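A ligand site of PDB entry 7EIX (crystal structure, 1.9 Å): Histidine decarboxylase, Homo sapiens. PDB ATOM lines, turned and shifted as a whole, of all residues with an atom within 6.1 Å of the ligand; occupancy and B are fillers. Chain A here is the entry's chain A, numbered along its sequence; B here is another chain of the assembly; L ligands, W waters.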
ATOM      1  N   TYR A  85      23.128  22.034 -27.978  1.00  0.00           N
ATOM      2  CA  TYR A  85      22.854  23.006 -29.043  1.00  0.00           C
ATOM      3  C   TYR A  85      23.557  22.491 -30.289  1.00  0.00           C
ATOM      4  O   TYR A  85      24.497  21.706 -30.232  1.00  0.00           O
ATOM      5  CB  TYR A  85      23.255  24.427 -28.646  1.00  0.00           C
ATOM      6  CG  TYR A  85      22.202  25.173 -27.860  1.00  0.00           C
ATOM      7  CD1 TYR A  85      20.870  25.158 -28.251  1.00  0.00           C
ATOM      8  CD2 TYR A  85      22.536  25.913 -26.724  1.00  0.00           C
ATOM      9  CE1 TYR A  85      19.884  25.830 -27.526  1.00  0.00           C
ATOM     10  CE2 TYR A  85      21.570  26.615 -26.020  1.00  0.00           C
ATOM     11  CZ  TYR A  85      20.233  26.569 -26.406  1.00  0.00           C
ATOM     12  OH  TYR A  85      19.245  27.262 -25.741  1.00  0.00           O
ATOM     13  N   SER A 152      38.174  30.418 -29.423  1.00  0.00           N
ATOM     14  CA  SER A 152      37.813  29.002 -29.667  1.00  0.00           C
ATOM     15  C   SER A 152      36.454  28.670 -29.095  1.00  0.00           C
ATOM     16  O   SER A 152      35.816  27.753 -29.629  1.00  0.00           O
ATOM     17  CB  SER A 152      38.860  28.095 -29.118  1.00  0.00           C
ATOM     18  OG  SER A 152      39.961  28.233 -29.974  1.00  0.00           O
ATOM     19  N   THR A 153      36.063  29.295 -28.003  1.00  0.00           N
ATOM     20  CA  THR A 153      34.839  28.926 -27.252  1.00  0.00           C
ATOM     21  C   THR A 153      34.208  30.168 -26.590  1.00  0.00           C
ATOM     22  O   THR A 153      34.906  31.173 -26.256  1.00  0.00           O
ATOM     23  CB  THR A 153      35.093  27.860 -26.161  1.00  0.00           C
ATOM     24  OG1 THR A 153      35.975  28.377 -25.170  1.00  0.00           O
ATOM     25  CG2 THR A 153      35.649  26.540 -26.658  1.00  0.00           C
ATOM     26  N   VAL A 154      32.893  30.098 -26.353  1.00  0.00           N
ATOM     27  CA  VAL A 154      32.246  31.099 -25.473  1.00  0.00           C
ATOM     28  C   VAL A 154      32.807  30.966 -24.053  1.00  0.00           C
ATOM     29  O   VAL A 154      33.022  31.991 -23.413  1.00  0.00           O
ATOM     30  CB  VAL A 154      30.717  30.978 -25.566  1.00  0.00           C
ATOM     31  CG1 VAL A 154      30.076  31.572 -24.345  1.00  0.00           C
ATOM     32  CG2 VAL A 154      30.275  31.670 -26.876  1.00  0.00           C
ATOM     33  N   SER A 155      33.030  29.740 -23.544  1.00  0.00           N
ATOM     34  CA  SER A 155      33.583  29.515 -22.192  1.00  0.00           C
ATOM     35  C   SER A 155      34.777  30.424 -21.981  1.00  0.00           C
ATOM     36  O   SER A 155      34.818  31.131 -20.945  1.00  0.00           O
ATOM     37  CB  SER A 155      33.994  28.072 -21.991  1.00  0.00           C
ATOM     38  OG  SER A 155      32.840  27.244 -22.061  1.00  0.00           O
ATOM     39  N   GLU A 156      35.773  30.348 -22.887  1.00  0.00           N
ATOM     40  CA  GLU A 156      37.017  31.157 -22.737  1.00  0.00           C
ATOM     41  C   GLU A 156      36.703  32.631 -22.913  1.00  0.00           C
ATOM     42  O   GLU A 156      37.338  33.416 -22.281  1.00  0.00           O
ATOM     43  CB  GLU A 156      38.095  30.833 -23.760  1.00  0.00           C
ATOM     44  CG  GLU A 156      38.727  29.502 -23.552  1.00  0.00           C
ATOM     45  CD  GLU A 156      39.379  29.064 -24.845  1.00  0.00           C
ATOM     46  OE1 GLU A 156      40.494  29.643 -25.121  1.00  0.00           O
ATOM     47  OE2 GLU A 156      38.675  28.251 -25.636  1.00  0.00           O
ATOM     48  N   HIS A 198      25.168  29.166 -18.005  1.00  0.00           N
ATOM     49  CA  HIS A 198      25.990  28.034 -18.459  1.00  0.00           C
ATOM     50  C   HIS A 198      27.090  27.803 -17.425  1.00  0.00           C
ATOM     51  O   HIS A 198      27.589  28.821 -16.804  1.00  0.00           O
ATOM     52  CB  HIS A 198      26.506  28.362 -19.868  1.00  0.00           C
ATOM     53  CG  HIS A 198      27.243  27.228 -20.476  1.00  0.00           C
ATOM     54  ND1 HIS A 198      28.626  27.197 -20.478  1.00  0.00           N
ATOM     55  CD2 HIS A 198      26.805  26.048 -20.990  1.00  0.00           C
ATOM     56  CE1 HIS A 198      29.008  26.040 -21.013  1.00  0.00           C
ATOM     57  NE2 HIS A 198      27.904  25.327 -21.362  1.00  0.00           N
ATOM     58  N   SER A 200      30.101  27.467 -17.688  1.00  0.00           N
ATOM     59  CA  SER A 200      31.340  28.228 -17.952  1.00  0.00           C
ATOM     60  C   SER A 200      31.442  29.453 -17.028  1.00  0.00           C
ATOM     61  O   SER A 200      32.569  29.910 -16.773  1.00  0.00           O
ATOM     62  CB  SER A 200      31.429  28.655 -19.379  1.00  0.00           C
ATOM     63  OG  SER A 200      30.234  29.298 -19.785  1.00  0.00           O
ATOM     64  N   THR A 248      22.645  36.409 -20.016  1.00  0.00           N
ATOM     65  CA  THR A 248      22.558  35.293 -20.982  1.00  0.00           C
ATOM     66  C   THR A 248      21.401  35.559 -21.937  1.00  0.00           C
ATOM     67  O   THR A 248      20.263  35.738 -21.468  1.00  0.00           O
ATOM     68  CB  THR A 248      22.497  33.944 -20.300  1.00  0.00           C
ATOM     69  OG1 THR A 248      23.599  33.819 -19.406  1.00  0.00           O
ATOM     70  CG2 THR A 248      22.598  32.811 -21.316  1.00  0.00           C
ATOM     71  N   LEU A 249      21.683  35.536 -23.226  1.00  0.00           N
ATOM     72  CA  LEU A 249      20.659  35.564 -24.315  1.00  0.00           C
ATOM     73  C   LEU A 249      20.617  34.156 -24.935  1.00  0.00           C
ATOM     74  O   LEU A 249      21.504  33.830 -25.790  1.00  0.00           O
ATOM     75  CB  LEU A 249      20.953  36.655 -25.335  1.00  0.00           C
ATOM     76  CG  LEU A 249      21.132  38.064 -24.783  1.00  0.00           C
ATOM     77  CD1 LEU A 249      21.277  39.088 -25.895  1.00  0.00           C
ATOM     78  CD2 LEU A 249      20.003  38.506 -23.873  1.00  0.00           C
ATOM     79  N   GLY A 250      19.648  33.359 -24.491  1.00  0.00           N
ATOM     80  CA  GLY A 250      19.467  31.965 -24.938  1.00  0.00           C
ATOM     81  C   GLY A 250      20.096  30.970 -23.994  1.00  0.00           C
ATOM     82  O   GLY A 250      21.099  30.289 -24.371  1.00  0.00           O
ATOM     83  N   THR A 251      19.554  30.820 -22.791  1.00  0.00           N
ATOM     84  CA  THR A 251      20.104  29.910 -21.768  1.00  0.00           C
ATOM     85  C   THR A 251      20.124  28.465 -22.335  1.00  0.00           C
ATOM     86  O   THR A 251      19.315  28.137 -23.190  1.00  0.00           O
ATOM     87  CB  THR A 251      19.338  30.019 -20.444  1.00  0.00           C
ATOM     88  OG1 THR A 251      18.004  29.545 -20.674  1.00  0.00           O
ATOM     89  CG2 THR A 251      19.360  31.421 -19.884  1.00  0.00           C
ATOM     90  N   THR A 252      21.036  27.632 -21.866  1.00  0.00           N
ATOM     91  CA  THR A 252      21.208  26.230 -22.327  1.00  0.00           C
ATOM     92  C   THR A 252      19.943  25.417 -22.022  1.00  0.00           C
ATOM     93  O   THR A 252      19.540  24.717 -22.895  1.00  0.00           O
ATOM     94  CB  THR A 252      22.434  25.571 -21.682  1.00  0.00           C
ATOM     95  OG1 THR A 252      23.582  26.333 -22.043  1.00  0.00           O
ATOM     96  CG2 THR A 252      22.652  24.162 -22.186  1.00  0.00           C
ATOM     97  N   ASP A 277      26.466  36.686 -22.949  1.00  0.00           N
ATOM     98  CA  ASP A 277      26.655  35.308 -23.456  1.00  0.00           C
ATOM     99  C   ASP A 277      25.456  35.004 -24.332  1.00  0.00           C
ATOM    100  O   ASP A 277      24.350  34.749 -23.787  1.00  0.00           O
ATOM    101  CB  ASP A 277      26.801  34.290 -22.329  1.00  0.00           C
ATOM    102  CG  ASP A 277      26.796  32.845 -22.785  1.00  0.00           C
ATOM    103  OD1 ASP A 277      26.645  32.613 -24.009  1.00  0.00           O
ATOM    104  OD2 ASP A 277      26.898  31.973 -21.889  1.00  0.00           O
ATOM    105  N   ALA A 278      25.638  35.066 -25.633  1.00  0.00           N
ATOM    106  CA  ALA A 278      24.592  34.766 -26.617  1.00  0.00           C
ATOM    107  C   ALA A 278      25.036  33.576 -27.455  1.00  0.00           C
ATOM    108  O   ALA A 278      24.754  33.593 -28.666  1.00  0.00           O
ATOM    109  CB  ALA A 278      24.347  35.988 -27.454  1.00  0.00           C
ATOM    110  N   ALA A 279      25.715  32.599 -26.841  1.00  0.00           N
ATOM    111  CA  ALA A 279      26.403  31.498 -27.565  1.00  0.00           C
ATOM    112  C   ALA A 279      25.572  30.966 -28.749  1.00  0.00           C
ATOM    113  O   ALA A 279      26.105  30.856 -29.899  1.00  0.00           O
ATOM    114  CB  ALA A 279      26.720  30.382 -26.604  1.00  0.00           C
ATOM    115  N   TYR A 280      24.346  30.501 -28.451  1.00  0.00           N
ATOM    116  CA  TYR A 280      23.442  29.863 -29.433  1.00  0.00           C
ATOM    117  C   TYR A 280      22.647  30.962 -30.132  1.00  0.00           C
ATOM    118  O   TYR A 280      22.693  31.044 -31.372  1.00  0.00           O
ATOM    119  CB  TYR A 280      22.488  28.901 -28.717  1.00  0.00           C
ATOM    120  CG  TYR A 280      21.283  28.518 -29.546  1.00  0.00           C
ATOM    121  CD1 TYR A 280      21.430  27.776 -30.715  1.00  0.00           C
ATOM    122  CD2 TYR A 280      20.005  28.773 -29.098  1.00  0.00           C
ATOM    123  CE1 TYR A 280      20.333  27.370 -31.473  1.00  0.00           C
ATOM    124  CE2 TYR A 280      18.899  28.399 -29.843  1.00  0.00           C
ATOM    125  CZ  TYR A 280      19.057  27.677 -31.022  1.00  0.00           C
ATOM    126  OH  TYR A 280      17.931  27.243 -31.686  1.00  0.00           O
ATOM    127  N   ASN A 306      28.505  32.031 -30.808  1.00  0.00           N
ATOM    128  CA  ASN A 306      29.195  30.951 -31.538  1.00  0.00           C
ATOM    129  C   ASN A 306      28.613  30.799 -32.919  1.00  0.00           C
ATOM    130  O   ASN A 306      27.610  30.109 -33.069  1.00  0.00           O
ATOM    131  CB  ASN A 306      29.081  29.614 -30.831  1.00  0.00           C
ATOM    132  CG  ASN A 306      30.096  29.431 -29.738  1.00  0.00           C
ATOM    133  OD1 ASN A 306      31.134  30.104 -29.675  1.00  0.00           O
ATOM    134  ND2 ASN A 306      29.757  28.540 -28.832  1.00  0.00           N
ATOM    135  N   SER A 308      29.959  28.702 -34.504  1.00  0.00           N
ATOM    136  CA  SER A 308      30.206  27.232 -34.422  1.00  0.00           C
ATOM    137  C   SER A 308      29.023  26.482 -33.809  1.00  0.00           C
ATOM    138  O   SER A 308      29.142  25.245 -33.629  1.00  0.00           O
ATOM    139  CB  SER A 308      31.417  26.921 -33.615  1.00  0.00           C
ATOM    140  OG  SER A 308      31.226  27.359 -32.256  1.00  0.00           O
ATOM    141  N   LYS A 309      27.935  27.173 -33.472  1.00  0.00           N
ATOM    142  CA  LYS A 309      26.692  26.473 -33.054  1.00  0.00           C
ATOM    143  C   LYS A 309      25.746  26.473 -34.251  1.00  0.00           C
ATOM    144  O   LYS A 309      25.497  25.377 -34.786  1.00  0.00           O
ATOM    145  CB  LYS A 309      26.080  27.086 -31.806  1.00  0.00           C
ATOM    146  CG  LYS A 309      26.793  26.689 -30.536  1.00  0.00           C
ATOM    147  CD  LYS A 309      26.110  27.009 -29.231  1.00  0.00           C
ATOM    148  CE  LYS A 309      26.902  26.399 -28.099  1.00  0.00           C
ATOM    149  NZ  LYS A 309      26.261  26.639 -26.834  1.00  0.00           N
ATOM    150  N   PHE A 315      33.499  23.881 -35.754  1.00  0.00           N
ATOM    151  CA  PHE A 315      34.212  24.271 -34.516  1.00  0.00           C
ATOM    152  C   PHE A 315      35.710  24.141 -34.774  1.00  0.00           C
ATOM    153  O   PHE A 315      36.094  23.127 -35.347  1.00  0.00           O
ATOM    154  CB  PHE A 315      33.716  23.370 -33.391  1.00  0.00           C
ATOM    155  CG  PHE A 315      34.306  23.672 -32.038  1.00  0.00           C
ATOM    156  CD1 PHE A 315      33.650  24.459 -31.126  1.00  0.00           C
ATOM    157  CD2 PHE A 315      35.523  23.102 -31.666  1.00  0.00           C
ATOM    158  CE1 PHE A 315      34.201  24.716 -29.881  1.00  0.00           C
ATOM    159  CE2 PHE A 315      36.105  23.396 -30.446  1.00  0.00           C
ATOM    160  CZ  PHE A 315      35.425  24.168 -29.528  1.00  0.00           C
ATOM    161  N   THR A 318      34.374  31.246 -32.377  1.00  0.00           N
ATOM    162  CA  THR A 318      33.604  32.073 -31.439  1.00  0.00           C
ATOM    163  C   THR A 318      33.902  33.522 -31.743  1.00  0.00           C
ATOM    164  O   THR A 318      35.101  33.854 -31.822  1.00  0.00           O
ATOM    165  CB  THR A 318      33.923  31.761 -29.970  1.00  0.00           C
ATOM    166  OG1 THR A 318      33.584  30.388 -29.739  1.00  0.00           O
ATOM    167  CG2 THR A 318      33.170  32.678 -29.036  1.00  0.00           C
ATOM    168  N   LEU B 106      31.678  17.407 -30.965  1.00  0.00           N
ATOM    169  CA  LEU B 106      32.332  18.002 -29.779  1.00  0.00           C
ATOM    170  C   LEU B 106      32.511  16.915 -28.742  1.00  0.00           C
ATOM    171  O   LEU B 106      31.607  16.046 -28.625  1.00  0.00           O
ATOM    172  CB  LEU B 106      31.504  19.140 -29.221  1.00  0.00           C
ATOM    173  CG  LEU B 106      31.167  20.247 -30.221  1.00  0.00           C
ATOM    174  CD1 LEU B 106      30.232  21.266 -29.574  1.00  0.00           C
ATOM    175  CD2 LEU B 106      32.441  20.876 -30.706  1.00  0.00           C
ATOM    176  N   PRO B 356      38.105  25.469 -21.299  1.00  0.00           N
ATOM    177  CA  PRO B 356      36.741  25.525 -21.812  1.00  0.00           C
ATOM    178  C   PRO B 356      35.956  24.222 -21.578  1.00  0.00           C
ATOM    179  O   PRO B 356      36.441  23.345 -20.966  1.00  0.00           O
ATOM    180  CB  PRO B 356      36.952  25.842 -23.311  1.00  0.00           C
ATOM    181  CG  PRO B 356      38.281  25.205 -23.643  1.00  0.00           C
ATOM    182  CD  PRO B 356      39.110  25.257 -22.360  1.00  0.00           C
ATOM    183  N   LEU B 357      34.701  24.216 -21.976  1.00  0.00           N
ATOM    184  CA  LEU B 357      33.846  23.018 -22.008  1.00  0.00           C
ATOM    185  C   LEU B 357      34.087  22.298 -23.345  1.00  0.00           C
ATOM    186  O   LEU B 357      34.602  21.183 -23.340  1.00  0.00           O
ATOM    187  CB  LEU B 357      32.393  23.491 -21.861  1.00  0.00           C
ATOM    188  CG  LEU B 357      31.299  22.419 -21.836  1.00  0.00           C
ATOM    189  CD1 LEU B 357      30.945  22.059 -20.402  1.00  0.00           C
ATOM    190  CD2 LEU B 357      30.035  22.903 -22.572  1.00  0.00           C
ATOM    191  N   SER B 358      33.692  22.923 -24.458  1.00  0.00           N
ATOM    192  CA  SER B 358      33.730  22.319 -25.822  1.00  0.00           C
ATOM    193  C   SER B 358      35.192  22.015 -26.171  1.00  0.00           C
ATOM    194  O   SER B 358      36.068  22.778 -25.779  1.00  0.00           O
ATOM    195  CB  SER B 358      33.138  23.242 -26.847  1.00  0.00           C
ATOM    196  OG  SER B 358      31.736  23.183 -26.773  1.00  0.00           O
HETATM  197  N1  LIG L   1      26.604  29.579 -22.865  1.00  0.00           N
HETATM  198  C1  LIG L   1      25.515  29.219 -23.534  1.00  0.00           C
HETATM  199  C2  LIG L   1      24.239  29.948 -23.277  1.00  0.00           C
HETATM  200  C3  LIG L   1      25.605  28.149 -24.460  1.00  0.00           C
HETATM  201  O1  LIG L   1      24.529  27.752 -25.179  1.00  0.00           O
HETATM  202  C4  LIG L   1      26.843  27.516 -24.652  1.00  0.00           C
HETATM  203  C5  LIG L   1      26.913  26.498 -25.667  1.00  0.00           C
HETATM  204  C6  LIG L   1      27.970  27.956 -23.965  1.00  0.00           C
HETATM  205  C7  LIG L   1      27.786  28.975 -23.071  1.00  0.00           C
HETATM  206  C8  LIG L   1      29.314  27.291 -24.087  1.00  0.00           C
HETATM  207  O2  LIG L   1      29.969  27.546 -25.362  1.00  0.00           O
HETATM  208  P1  LIG L   1      31.370  26.841 -25.676  1.00  0.00           P
HETATM  209  O3  LIG L   1      31.735  27.543 -26.960  1.00  0.00           O
HETATM  210  O4  LIG L   1      31.035  25.396 -25.782  1.00  0.00           O
HETATM  211  O5  LIG L   1      32.240  27.126 -24.534  1.00  0.00           O
HETATM  212  O   HOH W   1      31.152  25.563 -28.919  1.00  0.00           O
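The side-chain amino group (NZ) of Lys 309 is bonded to a carbon (C5) of the ligand, at 1.3 Å.
N of Val 154 is in hydrogen-bond range of O3 of the ligand (2.9 Å).
The side-chain carboxylate (OD2) of Asp 277 is in hydrogen-bond range of a nitrogen (N1) of the ligand (2.6 Å).
The backbone NH of Ser 155 is in hydrogen-bond range of an oxygen (O5) of the ligand (2.9 Å).
The side-chain hydroxyl of Ser 155 sits at hydrogen-bond distance from an oxygen (O5) of the ligand.
An oxygen (O4) of the ligand lies within hydrogen-bond range of the side-chain hydroxyl (OG) of Ser 358 of chain B.
An oxygen (O3) of the ligand sits at hydrogen-bond distance from the side-chain amide nitrogen (ND2) of Asn 306 (2.9 Å).
OE2 of Glu 156 lies within hydrogen-bond range of OG1 of Thr 153 (2.7 Å).
The side-chain hydroxyl (OG1) of Thr 318 lies close to the backbone NH (N) of Thr 153 (3.2 Å).
The backbone NH (N) of Asn 306 is in hydrogen-bond range of the backbone carbonyl oxygen (O) of Ala 279 (2.8 Å).
OG1 of Thr 318 is in hydrogen-bond range of N of Val 154 (3.5 Å).
A ring nitrogen (ND1) of His 198 lies within hydrogen-bond range of the side-chain hydroxyl of Ser 200.
OH of Tyr 85 sits at hydrogen-bond distance from O of Thr 251 (2.7 Å).
OD1 of Asp 277 lies within hydrogen-bond range of N of Ala 279.
The backbone carbonyl oxygen of Asp 277 sits at hydrogen-bond distance from the backbone NH of Leu 249 (2.8 Å).
Tyr 85 touches the ligand (CD2 to O1, 3.1 Å).
Thr 153 touches the ligand (CB to O5, 3.4 Å).
CG of His 198 touches C7 of the ligand, at 3.2 Å.
Thr 248 touches the ligand (CG2 to C2, 3.8 Å).
O of Gly 250 touches C2 of the ligand, 3.3 Å away.
Thr 252 touches the ligand (OG1 to O1, 3.6 Å).
Ala 279 touches the ligand.
Hydrophobic or aromatic side chains within 4 Å of the ligand: Tyr 85, Val 154, His 198 and Ala 279.
13 residues have an atom within 4 Å of the ligand: Tyr 85, Thr 153, Val 154, Ser 155, His 198, Thr 248, Gly 250, Thr 252, Asp 277, Ala 279, Asn 306, Lys 309 and Ser 358 of chain B.
Water W1 lies within hydrogen-bond range of an oxygen (O3) of the ligand, the side-chain hydroxyl (OG) of Ser 358 of chain B and the side-chain amide nitrogen (ND2) of Asn 306.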
